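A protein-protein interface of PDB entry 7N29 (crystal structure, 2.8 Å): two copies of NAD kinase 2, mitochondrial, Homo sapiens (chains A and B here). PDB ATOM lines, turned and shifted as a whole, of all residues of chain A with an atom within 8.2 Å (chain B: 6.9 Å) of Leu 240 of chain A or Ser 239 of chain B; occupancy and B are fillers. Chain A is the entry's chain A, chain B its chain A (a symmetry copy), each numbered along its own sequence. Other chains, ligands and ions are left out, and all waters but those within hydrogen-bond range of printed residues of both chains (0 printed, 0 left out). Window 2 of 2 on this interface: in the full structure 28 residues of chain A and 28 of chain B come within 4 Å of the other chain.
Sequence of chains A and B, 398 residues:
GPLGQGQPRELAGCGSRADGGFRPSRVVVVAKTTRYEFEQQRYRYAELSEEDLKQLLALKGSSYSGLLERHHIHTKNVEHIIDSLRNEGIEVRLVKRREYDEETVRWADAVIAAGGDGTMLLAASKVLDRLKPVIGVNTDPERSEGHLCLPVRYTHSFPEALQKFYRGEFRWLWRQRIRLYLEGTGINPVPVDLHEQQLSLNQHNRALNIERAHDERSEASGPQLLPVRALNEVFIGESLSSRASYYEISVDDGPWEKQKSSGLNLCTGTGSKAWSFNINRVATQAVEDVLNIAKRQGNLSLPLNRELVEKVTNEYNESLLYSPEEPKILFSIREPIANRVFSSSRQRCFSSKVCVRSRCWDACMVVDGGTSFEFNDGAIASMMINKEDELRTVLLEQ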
ATOM      1  N   PHE A 235      -9.170  19.075  37.597  1.00  0.00           N
ATOM      2  CA  PHE A 235      -9.045  20.452  37.147  1.00  0.00           C
ATOM      3  C   PHE A 235     -10.415  21.038  36.840  1.00  0.00           C
ATOM      4  O   PHE A 235     -11.191  20.446  36.081  1.00  0.00           O
ATOM      5  CB  PHE A 235      -8.185  20.556  35.896  1.00  0.00           C
ATOM      6  CG  PHE A 235      -8.121  21.933  35.360  1.00  0.00           C
ATOM      7  CD1 PHE A 235      -7.300  22.869  35.948  1.00  0.00           C
ATOM      8  CD2 PHE A 235      -8.895  22.303  34.281  1.00  0.00           C
ATOM      9  CE1 PHE A 235      -7.247  24.150  35.447  1.00  0.00           C
ATOM     10  CE2 PHE A 235      -8.847  23.585  33.780  1.00  0.00           C
ATOM     11  CZ  PHE A 235      -8.017  24.497  34.356  1.00  0.00           C
ATOM     12  N   GLY A 237     -12.411  24.519  35.611  1.00  0.00           N
ATOM     13  CA  GLY A 237     -12.234  25.828  35.003  1.00  0.00           C
ATOM     14  C   GLY A 237     -12.953  25.929  33.674  1.00  0.00           C
ATOM     15  O   GLY A 237     -13.561  24.974  33.180  1.00  0.00           O
ATOM     16  N   GLU A 238     -12.898  27.118  33.107  1.00  0.00           N
ATOM     17  CA  GLU A 238     -13.572  27.339  31.838  1.00  0.00           C
ATOM     18  C   GLU A 238     -12.955  26.470  30.753  1.00  0.00           C
ATOM     19  O   GLU A 238     -11.749  26.257  30.702  1.00  0.00           O
ATOM     20  CB  GLU A 238     -13.501  28.820  31.446  1.00  0.00           C
ATOM     21  CG  GLU A 238     -14.573  29.647  32.105  1.00  0.00           C
ATOM     22  CD  GLU A 238     -15.872  29.629  31.330  1.00  0.00           C
ATOM     23  OE1 GLU A 238     -16.830  30.278  31.757  1.00  0.00           O
ATOM     24  OE2 GLU A 238     -15.937  28.991  30.262  1.00  0.00           O
ATOM     25  N   SER A 239     -13.803  25.967  29.877  1.00  0.00           N
ATOM     26  CA  SER A 239     -13.342  25.069  28.836  1.00  0.00           C
ATOM     27  C   SER A 239     -12.226  25.695  27.998  1.00  0.00           C
ATOM     28  O   SER A 239     -11.376  24.986  27.468  1.00  0.00           O
ATOM     29  CB  SER A 239     -14.547  24.686  27.984  1.00  0.00           C
ATOM     30  OG  SER A 239     -14.357  23.464  27.320  1.00  0.00           O
ATOM     31  N   LEU A 240     -12.192  27.017  27.886  1.00  0.00           N
ATOM     32  CA  LEU A 240     -11.302  27.714  26.966  1.00  0.00           C
ATOM     33  C   LEU A 240     -10.153  28.347  27.736  1.00  0.00           C
ATOM     34  O   LEU A 240     -10.359  28.926  28.805  1.00  0.00           O
ATOM     35  CB  LEU A 240     -12.084  28.775  26.188  1.00  0.00           C
ATOM     36  CG  LEU A 240     -11.763  29.168  24.742  1.00  0.00           C
ATOM     37  CD1 LEU A 240     -11.746  27.970  23.811  1.00  0.00           C
ATOM     38  CD2 LEU A 240     -12.792  30.145  24.272  1.00  0.00           C
ATOM     39  N   SER A 241      -8.942  28.251  27.177  1.00  0.00           N
ATOM     40  CA  SER A 241      -7.729  28.537  27.945  1.00  0.00           C
ATOM     41  C   SER A 241      -7.686  29.974  28.443  1.00  0.00           C
ATOM     42  O   SER A 241      -7.198  30.240  29.551  1.00  0.00           O
ATOM     43  CB  SER A 241      -6.495  28.263  27.100  1.00  0.00           C
ATOM     44  OG  SER A 241      -6.683  27.090  26.346  1.00  0.00           O
ATOM     45  N   SER A 242      -8.174  30.913  27.639  1.00  0.00           N
ATOM     46  CA  SER A 242      -7.921  32.326  27.853  1.00  0.00           C
ATOM     47  C   SER A 242      -9.044  33.040  28.592  1.00  0.00           C
ATOM     48  O   SER A 242      -8.989  34.258  28.740  1.00  0.00           O
ATOM     49  CB  SER A 242      -7.678  33.002  26.498  1.00  0.00           C
ATOM     50  OG  SER A 242      -8.780  32.806  25.637  1.00  0.00           O
ATOM     51  N   ARG A 243     -10.055  32.321  29.044  1.00  0.00           N
ATOM     52  CA  ARG A 243     -11.230  32.902  29.671  1.00  0.00           C
ATOM     53  C   ARG A 243     -11.178  32.577  31.158  1.00  0.00           C
ATOM     54  O   ARG A 243     -10.999  31.415  31.531  1.00  0.00           O
ATOM     55  CB  ARG A 243     -12.484  32.336  29.006  1.00  0.00           C
ATOM     56  CG  ARG A 243     -13.822  32.947  29.377  1.00  0.00           C
ATOM     57  CD  ARG A 243     -14.965  32.136  28.727  1.00  0.00           C
ATOM     58  NE  ARG A 243     -14.844  32.027  27.267  1.00  0.00           N
ATOM     59  CZ  ARG A 243     -15.756  31.466  26.468  1.00  0.00           C
ATOM     60  NH1 ARG A 243     -16.865  30.943  26.976  1.00  0.00           N
ATOM     61  NH2 ARG A 243     -15.567  31.435  25.158  1.00  0.00           N
ATOM     62  N   ALA A 244     -11.271  33.595  32.008  1.00  0.00           N
ATOM     63  CA  ALA A 244     -11.188  33.351  33.444  1.00  0.00           C
ATOM     64  C   ALA A 244     -12.462  32.702  33.957  1.00  0.00           C
ATOM     65  O   ALA A 244     -13.542  32.813  33.386  1.00  0.00           O
ATOM     66  CB  ALA A 244     -10.928  34.638  34.217  1.00  0.00           C
ATOM     67  N   SER A 245     -12.319  32.041  35.079  1.00  0.00           N
ATOM     68  CA  SER A 245     -13.362  31.222  35.656  1.00  0.00           C
ATOM     69  C   SER A 245     -13.890  31.922  36.896  1.00  0.00           C
ATOM     70  O   SER A 245     -13.149  32.638  37.579  1.00  0.00           O
ATOM     71  CB  SER A 245     -12.792  29.847  36.024  1.00  0.00           C
ATOM     72  OG  SER A 245     -12.249  29.215  34.880  1.00  0.00           O
ATOM     73  N   SER A 262      -7.848  31.489  36.866  1.00  0.00           N
ATOM     74  CA  SER A 262      -7.690  30.636  35.687  1.00  0.00           C
ATOM     75  C   SER A 262      -7.857  29.167  36.011  1.00  0.00           C
ATOM     76  O   SER A 262      -7.163  28.342  35.427  1.00  0.00           O
ATOM     77  CB  SER A 262      -6.341  30.883  35.037  1.00  0.00           C
ATOM     78  OG  SER A 262      -6.376  32.073  34.272  1.00  0.00           O
ATOM     79  N   ARG A 334      -5.405  28.500  40.719  1.00  0.00           N
ATOM     80  CA  ARG A 334      -4.463  28.783  39.649  1.00  0.00           C
ATOM     81  C   ARG A 334      -4.628  30.225  39.140  1.00  0.00           C
ATOM     82  O   ARG A 334      -5.668  30.581  38.573  1.00  0.00           O
ATOM     83  CB  ARG A 334      -4.685  27.748  38.570  1.00  0.00           C
ATOM     84  CG  ARG A 334      -3.764  27.817  37.446  1.00  0.00           C
ATOM     85  CD  ARG A 334      -4.148  26.679  36.576  1.00  0.00           C
ATOM     86  NE  ARG A 334      -3.285  26.624  35.429  1.00  0.00           N
ATOM     87  CZ  ARG A 334      -3.731  26.627  34.193  1.00  0.00           C
ATOM     88  NH1 ARG A 334      -5.035  26.676  33.980  1.00  0.00           N
ATOM     89  NH2 ARG A 334      -2.871  26.564  33.193  1.00  0.00           N
ATOM     90  N   ASP A 362     -19.189  28.299  30.272  1.00  0.00           N
ATOM     91  CA  ASP A 362     -18.835  27.096  29.509  1.00  0.00           C
ATOM     92  C   ASP A 362     -17.644  26.419  30.189  1.00  0.00           C
ATOM     93  O   ASP A 362     -16.506  26.394  29.733  1.00  0.00           O
ATOM     94  CB  ASP A 362     -18.548  27.426  28.040  1.00  0.00           C
ATOM     95  CG  ASP A 362     -17.881  26.269  27.285  1.00  0.00           C
ATOM     96  OD1 ASP A 362     -18.375  25.116  27.356  1.00  0.00           O
ATOM     97  OD2 ASP A 362     -16.840  26.525  26.629  1.00  0.00           O
ATOM     98  N   ALA A 363     -17.901  25.821  31.336  1.00  0.00           N
ATOM     99  CA  ALA A 363     -16.833  25.246  32.125  1.00  0.00           C
ATOM    100  C   ALA A 363     -16.929  23.730  32.110  1.00  0.00           C
ATOM    101  O   ALA A 363     -17.935  23.137  31.706  1.00  0.00           O
ATOM    102  CB  ALA A 363     -16.872  25.782  33.556  1.00  0.00           C
ATOM    103  N   CYS A 364     -15.875  23.119  32.635  1.00  0.00           N
ATOM    104  CA  CYS A 364     -15.670  21.684  32.601  1.00  0.00           C
ATOM    105  C   CYS A 364     -14.882  21.293  33.845  1.00  0.00           C
ATOM    106  O   CYS A 364     -14.158  22.112  34.419  1.00  0.00           O
ATOM    107  CB  CYS A 364     -14.869  21.271  31.369  1.00  0.00           C
ATOM    108  SG  CYS A 364     -13.201  22.050  31.429  1.00  0.00           S
ATOM    109  N   LEU B 194     -14.333  35.949  20.340  1.00  0.00           N
ATOM    110  CA  LEU B 194     -14.702  34.998  21.378  1.00  0.00           C
ATOM    111  C   LEU B 194     -15.974  35.418  22.093  1.00  0.00           C
ATOM    112  O   LEU B 194     -16.789  34.560  22.445  1.00  0.00           O
ATOM    113  CB  LEU B 194     -13.561  34.855  22.378  1.00  0.00           C
ATOM    114  CG  LEU B 194     -12.337  34.225  21.732  1.00  0.00           C
ATOM    115  CD1 LEU B 194     -11.153  34.162  22.707  1.00  0.00           C
ATOM    116  CD2 LEU B 194     -12.712  32.847  21.197  1.00  0.00           C
ATOM    117  N   GLN B 197     -19.011  33.694  20.527  1.00  0.00           N
ATOM    118  CA  GLN B 197     -18.886  32.224  20.438  1.00  0.00           C
ATOM    119  C   GLN B 197     -17.868  31.773  19.384  1.00  0.00           C
ATOM    120  O   GLN B 197     -16.996  30.934  19.660  1.00  0.00           O
ATOM    121  CB  GLN B 197     -20.246  31.555  20.180  1.00  0.00           C
ATOM    122  N   PHE B 235      -1.886  35.686  24.011  1.00  0.00           N
ATOM    123  CA  PHE B 235      -1.821  34.383  24.654  1.00  0.00           C
ATOM    124  C   PHE B 235      -1.780  33.276  23.611  1.00  0.00           C
ATOM    125  O   PHE B 235      -2.633  33.230  22.717  1.00  0.00           O
ATOM    126  CB  PHE B 235      -3.019  34.147  25.562  1.00  0.00           C
ATOM    127  CG  PHE B 235      -3.029  32.791  26.154  1.00  0.00           C
ATOM    128  CD1 PHE B 235      -2.216  32.495  27.224  1.00  0.00           C
ATOM    129  CD2 PHE B 235      -3.833  31.802  25.630  1.00  0.00           C
ATOM    130  CE1 PHE B 235      -2.226  31.231  27.769  1.00  0.00           C
ATOM    131  CE2 PHE B 235      -3.844  30.535  26.169  1.00  0.00           C
ATOM    132  CZ  PHE B 235      -3.050  30.259  27.240  1.00  0.00           C
ATOM    133  N   GLY B 237      -1.505  29.121  23.093  1.00  0.00           N
ATOM    134  CA  GLY B 237      -1.615  27.838  23.769  1.00  0.00           C
ATOM    135  C   GLY B 237      -2.754  27.009  23.212  1.00  0.00           C
ATOM    136  O   GLY B 237      -3.504  27.432  22.327  1.00  0.00           O
ATOM    137  N   GLU B 238      -2.859  25.801  23.728  1.00  0.00           N
ATOM    138  CA  GLU B 238      -3.902  24.906  23.254  1.00  0.00           C
ATOM    139  C   GLU B 238      -5.275  25.479  23.571  1.00  0.00           C
ATOM    140  O   GLU B 238      -5.500  26.077  24.618  1.00  0.00           O
ATOM    141  CB  GLU B 238      -3.741  23.517  23.881  1.00  0.00           C
ATOM    142  CG  GLU B 238      -2.741  22.661  23.149  1.00  0.00           C
ATOM    143  CD  GLU B 238      -3.358  21.928  21.978  1.00  0.00           C
ATOM    144  OE1 GLU B 238      -2.648  21.182  21.300  1.00  0.00           O
ATOM    145  OE2 GLU B 238      -4.574  22.064  21.745  1.00  0.00           O
ATOM    146  N   SER B 239      -6.198  25.288  22.649  1.00  0.00           N
ATOM    147  CA  SER B 239      -7.527  25.846  22.809  1.00  0.00           C
ATOM    148  C   SER B 239      -8.176  25.402  24.121  1.00  0.00           C
ATOM    149  O   SER B 239      -8.995  26.124  24.683  1.00  0.00           O
ATOM    150  CB  SER B 239      -8.354  25.432  21.597  1.00  0.00           C
ATOM    151  OG  SER B 239      -9.426  26.308  21.366  1.00  0.00           O
ATOM    152  N   LEU B 240      -7.808  24.238  24.641  1.00  0.00           N
ATOM    153  CA  LEU B 240      -8.488  23.624  25.774  1.00  0.00           C
ATOM    154  C   LEU B 240      -7.643  23.772  27.029  1.00  0.00           C
ATOM    155  O   LEU B 240      -6.424  23.591  26.989  1.00  0.00           O
ATOM    156  CB  LEU B 240      -8.765  22.148  25.477  1.00  0.00           C
ATOM    157  CG  LEU B 240      -9.995  21.399  26.000  1.00  0.00           C
ATOM    158  CD1 LEU B 240     -11.292  22.095  25.632  1.00  0.00           C
ATOM    159  CD2 LEU B 240      -9.994  20.018  25.426  1.00  0.00           C
ATOM    160  N   SER B 241      -8.299  24.085  28.151  1.00  0.00           N
ATOM    161  CA  SER B 241      -7.585  24.555  29.340  1.00  0.00           C
ATOM    162  C   SER B 241      -6.610  23.517  29.876  1.00  0.00           C
ATOM    163  O   SER B 241      -5.526  23.867  30.364  1.00  0.00           O
ATOM    164  CB  SER B 241      -8.573  24.925  30.435  1.00  0.00           C
ATOM    165  OG  SER B 241      -9.679  25.591  29.875  1.00  0.00           O
ATOM    166  N   SER B 242      -6.979  22.242  29.809  1.00  0.00           N
ATOM    167  CA  SER B 242      -6.295  21.197  30.547  1.00  0.00           C
ATOM    168  C   SER B 242      -5.257  20.449  29.722  1.00  0.00           C
ATOM    169  O   SER B 242      -4.687  19.476  30.209  1.00  0.00           O
ATOM    170  CB  SER B 242      -7.332  20.209  31.096  1.00  0.00           C
ATOM    171  OG  SER B 242      -8.110  19.668  30.048  1.00  0.00           O
ATOM    172  N   ARG B 243      -5.008  20.869  28.495  1.00  0.00           N
ATOM    173  CA  ARG B 243      -4.118  20.177  27.579  1.00  0.00           C
ATOM    174  C   ARG B 243      -2.857  21.016  27.425  1.00  0.00           C
ATOM    175  O   ARG B 243      -2.942  22.215  27.148  1.00  0.00           O
ATOM    176  CB  ARG B 243      -4.834  19.970  26.244  1.00  0.00           C
ATOM    177  CG  ARG B 243      -4.156  19.101  25.202  1.00  0.00           C
ATOM    178  CD  ARG B 243      -4.955  19.150  23.881  1.00  0.00           C
ATOM    179  NE  ARG B 243      -6.362  18.755  24.036  1.00  0.00           N
ATOM    180  CZ  ARG B 243      -7.228  18.620  23.029  1.00  0.00           C
ATOM    181  NH1 ARG B 243      -6.850  18.856  21.779  1.00  0.00           N
ATOM    182  NH2 ARG B 243      -8.473  18.237  23.266  1.00  0.00           N
ATOM    183  N   SER B 245       0.692  22.496  25.950  1.00  0.00           N
ATOM    184  CA  SER B 245       1.022  23.035  24.649  1.00  0.00           C
ATOM    185  C   SER B 245       2.471  22.696  24.344  1.00  0.00           C
ATOM    186  O   SER B 245       3.300  22.596  25.255  1.00  0.00           O
ATOM    187  CB  SER B 245       0.823  24.556  24.658  1.00  0.00           C
ATOM    188  OG  SER B 245      -0.513  24.878  24.996  1.00  0.00           O
ATOM    189  N   ASP B 362      -4.539  21.495  18.470  1.00  0.00           N
ATOM    190  CA  ASP B 362      -5.710  22.378  18.403  1.00  0.00           C
ATOM    191  C   ASP B 362      -5.421  23.635  19.226  1.00  0.00           C
ATOM    192  O   ASP B 362      -5.950  23.899  20.300  1.00  0.00           O
ATOM    193  CB  ASP B 362      -6.981  21.662  18.873  1.00  0.00           C
ATOM    194  CG  ASP B 362      -8.154  22.621  19.114  1.00  0.00           C
ATOM    195  OD1 ASP B 362      -8.460  23.460  18.231  1.00  0.00           O
ATOM    196  OD2 ASP B 362      -8.761  22.535  20.211  1.00  0.00           O
ATOM    197  N   ALA B 363      -4.548  24.474  18.704  1.00  0.00           N
ATOM    198  CA  ALA B 363      -4.111  25.640  19.443  1.00  0.00           C
ATOM    199  C   ALA B 363      -4.661  26.903  18.803  1.00  0.00           C
ATOM    200  O   ALA B 363      -5.164  26.904  17.675  1.00  0.00           O
ATOM    201  CB  ALA B 363      -2.585  25.686  19.522  1.00  0.00           C
ATOM    202  N   CYS B 364      -4.481  27.996  19.531  1.00  0.00           N
ATOM    203  CA  CYS B 364      -5.044  29.291  19.200  1.00  0.00           C
ATOM    204  C   CYS B 364      -4.095  30.363  19.720  1.00  0.00           C
ATOM    205  O   CYS B 364      -3.330  30.129  20.660  1.00  0.00           O
ATOM    206  CB  CYS B 364      -6.406  29.485  19.863  1.00  0.00           C
ATOM    207  SG  CYS B 364      -6.211  29.435  21.694  1.00  0.00           S
ATOM    208  N   VAL B 366      -4.884  34.052  21.302  1.00  0.00           N
ATOM    209  CA  VAL B 366      -5.954  34.925  21.759  1.00  0.00           C
ATOM    210  C   VAL B 366      -5.363  36.292  22.081  1.00  0.00           C
ATOM    211  O   VAL B 366      -4.463  36.410  22.927  1.00  0.00           O
ATOM    212  CB  VAL B 366      -6.687  34.331  22.967  1.00  0.00           C
ATOM    213  CG1 VAL B 366      -7.661  35.350  23.520  1.00  0.00           C
ATOM    214  CG2 VAL B 366      -7.407  33.079  22.558  1.00  0.00           C
ATOM    215  N   SER B 372      -9.522  35.514  18.570  1.00  0.00           N
ATOM    216  CA  SER B 372      -8.802  34.250  18.534  1.00  0.00           C
ATOM    217  C   SER B 372      -8.378  33.914  17.105  1.00  0.00           C
ATOM    218  O   SER B 372      -9.114  34.185  16.153  1.00  0.00           O
ATOM    219  CB  SER B 372      -9.657  33.141  19.104  1.00  0.00           C
ATOM    220  OG  SER B 372      -8.955  31.925  19.063  1.00  0.00           O
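Glu 238 of chain A touches Ser 241 of chain B, and with the chains exchanged Ser 241 of chain A touches Glu 238 of chain B.
Ser 239 of chain A touches its own counterpart, Ser 239 of chain B.
Ser 239 of chain A touches Leu 240 of chain B, and with the chains exchanged Leu 240 of chain A touches Ser 239 of chain B.
Leu 240 of chain A touches Ser 241 of chain B, and with the chains exchanged Ser 241 of chain A touches Leu 240 of chain B.
12 positions are printed for both chains.
Printed residues of chain A that touch a printed residue of chain B: Phe 235, Glu 238, Ser 239, Leu 240, Ser 241 and Ser 242.
Hydrophobic or aromatic side chains of chain A that line the printed part of chain B: Phe 235 and Leu 240.
Of the 16 printed residues of chain B, 6 touch a printed residue of chain A.
Hydrophobic or aromatic side chains of chain B that line the printed part of chain A: Phe 235, Leu 240 and Val 366.
NH1 of Arg 243 of chain A is in salt-bridge range of OE2 of Glu 238 of chain A (3.9 Å).
N of Glu 238 of chain A sits at hydrogen-bond distance from OG of Ser 245 of chain A, at 2.8 Å.
OE2 of Glu 238 of chain A lies close to N of Asp 362 of chain A, at 3.3 Å.
The backbone NH of Ser 239 of chain A is in hydrogen-bond range of the backbone carbonyl oxygen of Asp 362 of chain A (2.7 Å).
The backbone NH (N) of Glu 238 of chain B lies within hydrogen-bond range of the side-chain hydroxyl (OG) of Ser 245 of chain B, 2.8 Å away.
The backbone NH (N) of Asp 362 of chain B sits close to the side-chain carboxylate (OE2) of Glu 238 of chain B, 3.3 Å away.
The backbone carbonyl oxygen (O) of Ser 239 of chain A sits at hydrogen-bond distance from the side-chain hydroxyl (OG) of Ser 241 of chain B, 3.0 Å away.
O of Ser 239 of chain B lies within hydrogen-bond range of OG of Ser 241 of chain A (3.0 Å).
OG of Ser 241 of chain B lies close to O of Glu 238 of chain A (2.3 Å).
The backbone carbonyl oxygen (O) of Glu 238 of chain B lies close to the side-chain hydroxyl (OG) of Ser 241 of chain A.
Among the printed residues, pairs that only touch across the chains: Ser 242 of chain A with Val 366 of chain B, Ser 239 of chain A with Leu 240 of chain B, Leu 240 of chain A with Ser 239 of chain B, Leu 240 of chain A with Ser 241 of chain B, Ser 241 of chain A with Leu 240 of chain B, Ser 241 of chain A with Phe 235 of chain B, Phe 235 of chain A with Ser 241 of chain B, Ser 239 of chain A with Ser 239 of chain B and Ser 241 of chain A with Ser 241 of chain B.
Leu 240 of chain A touches just these residues of chain B: Ser 239 and Ser 241.
Ser 239 of chain B touches just these residues of chain A: Ser 239 (3.8 Å), Leu 240 (3.4 Å) and Ser 241 (3.0 Å).
Of the printed residues of chain B, Glu 238 of chain A touches Ser 241.
Of the printed residues of chain A, Phe 235 of chain B touches Ser 241.
Ser 245 of chain A touches none of the printed residues of chain B.
Leu 194 of chain B touches none of the printed residues of chain A.
The nearest residue of chain A that does not touch Ser 239 of chain B is Ser 242 of chain A (5.7 Å).
The nearest printed residue of chain A that does not touch Val 366 of chain B is Leu 240 of chain A (6.2 Å).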
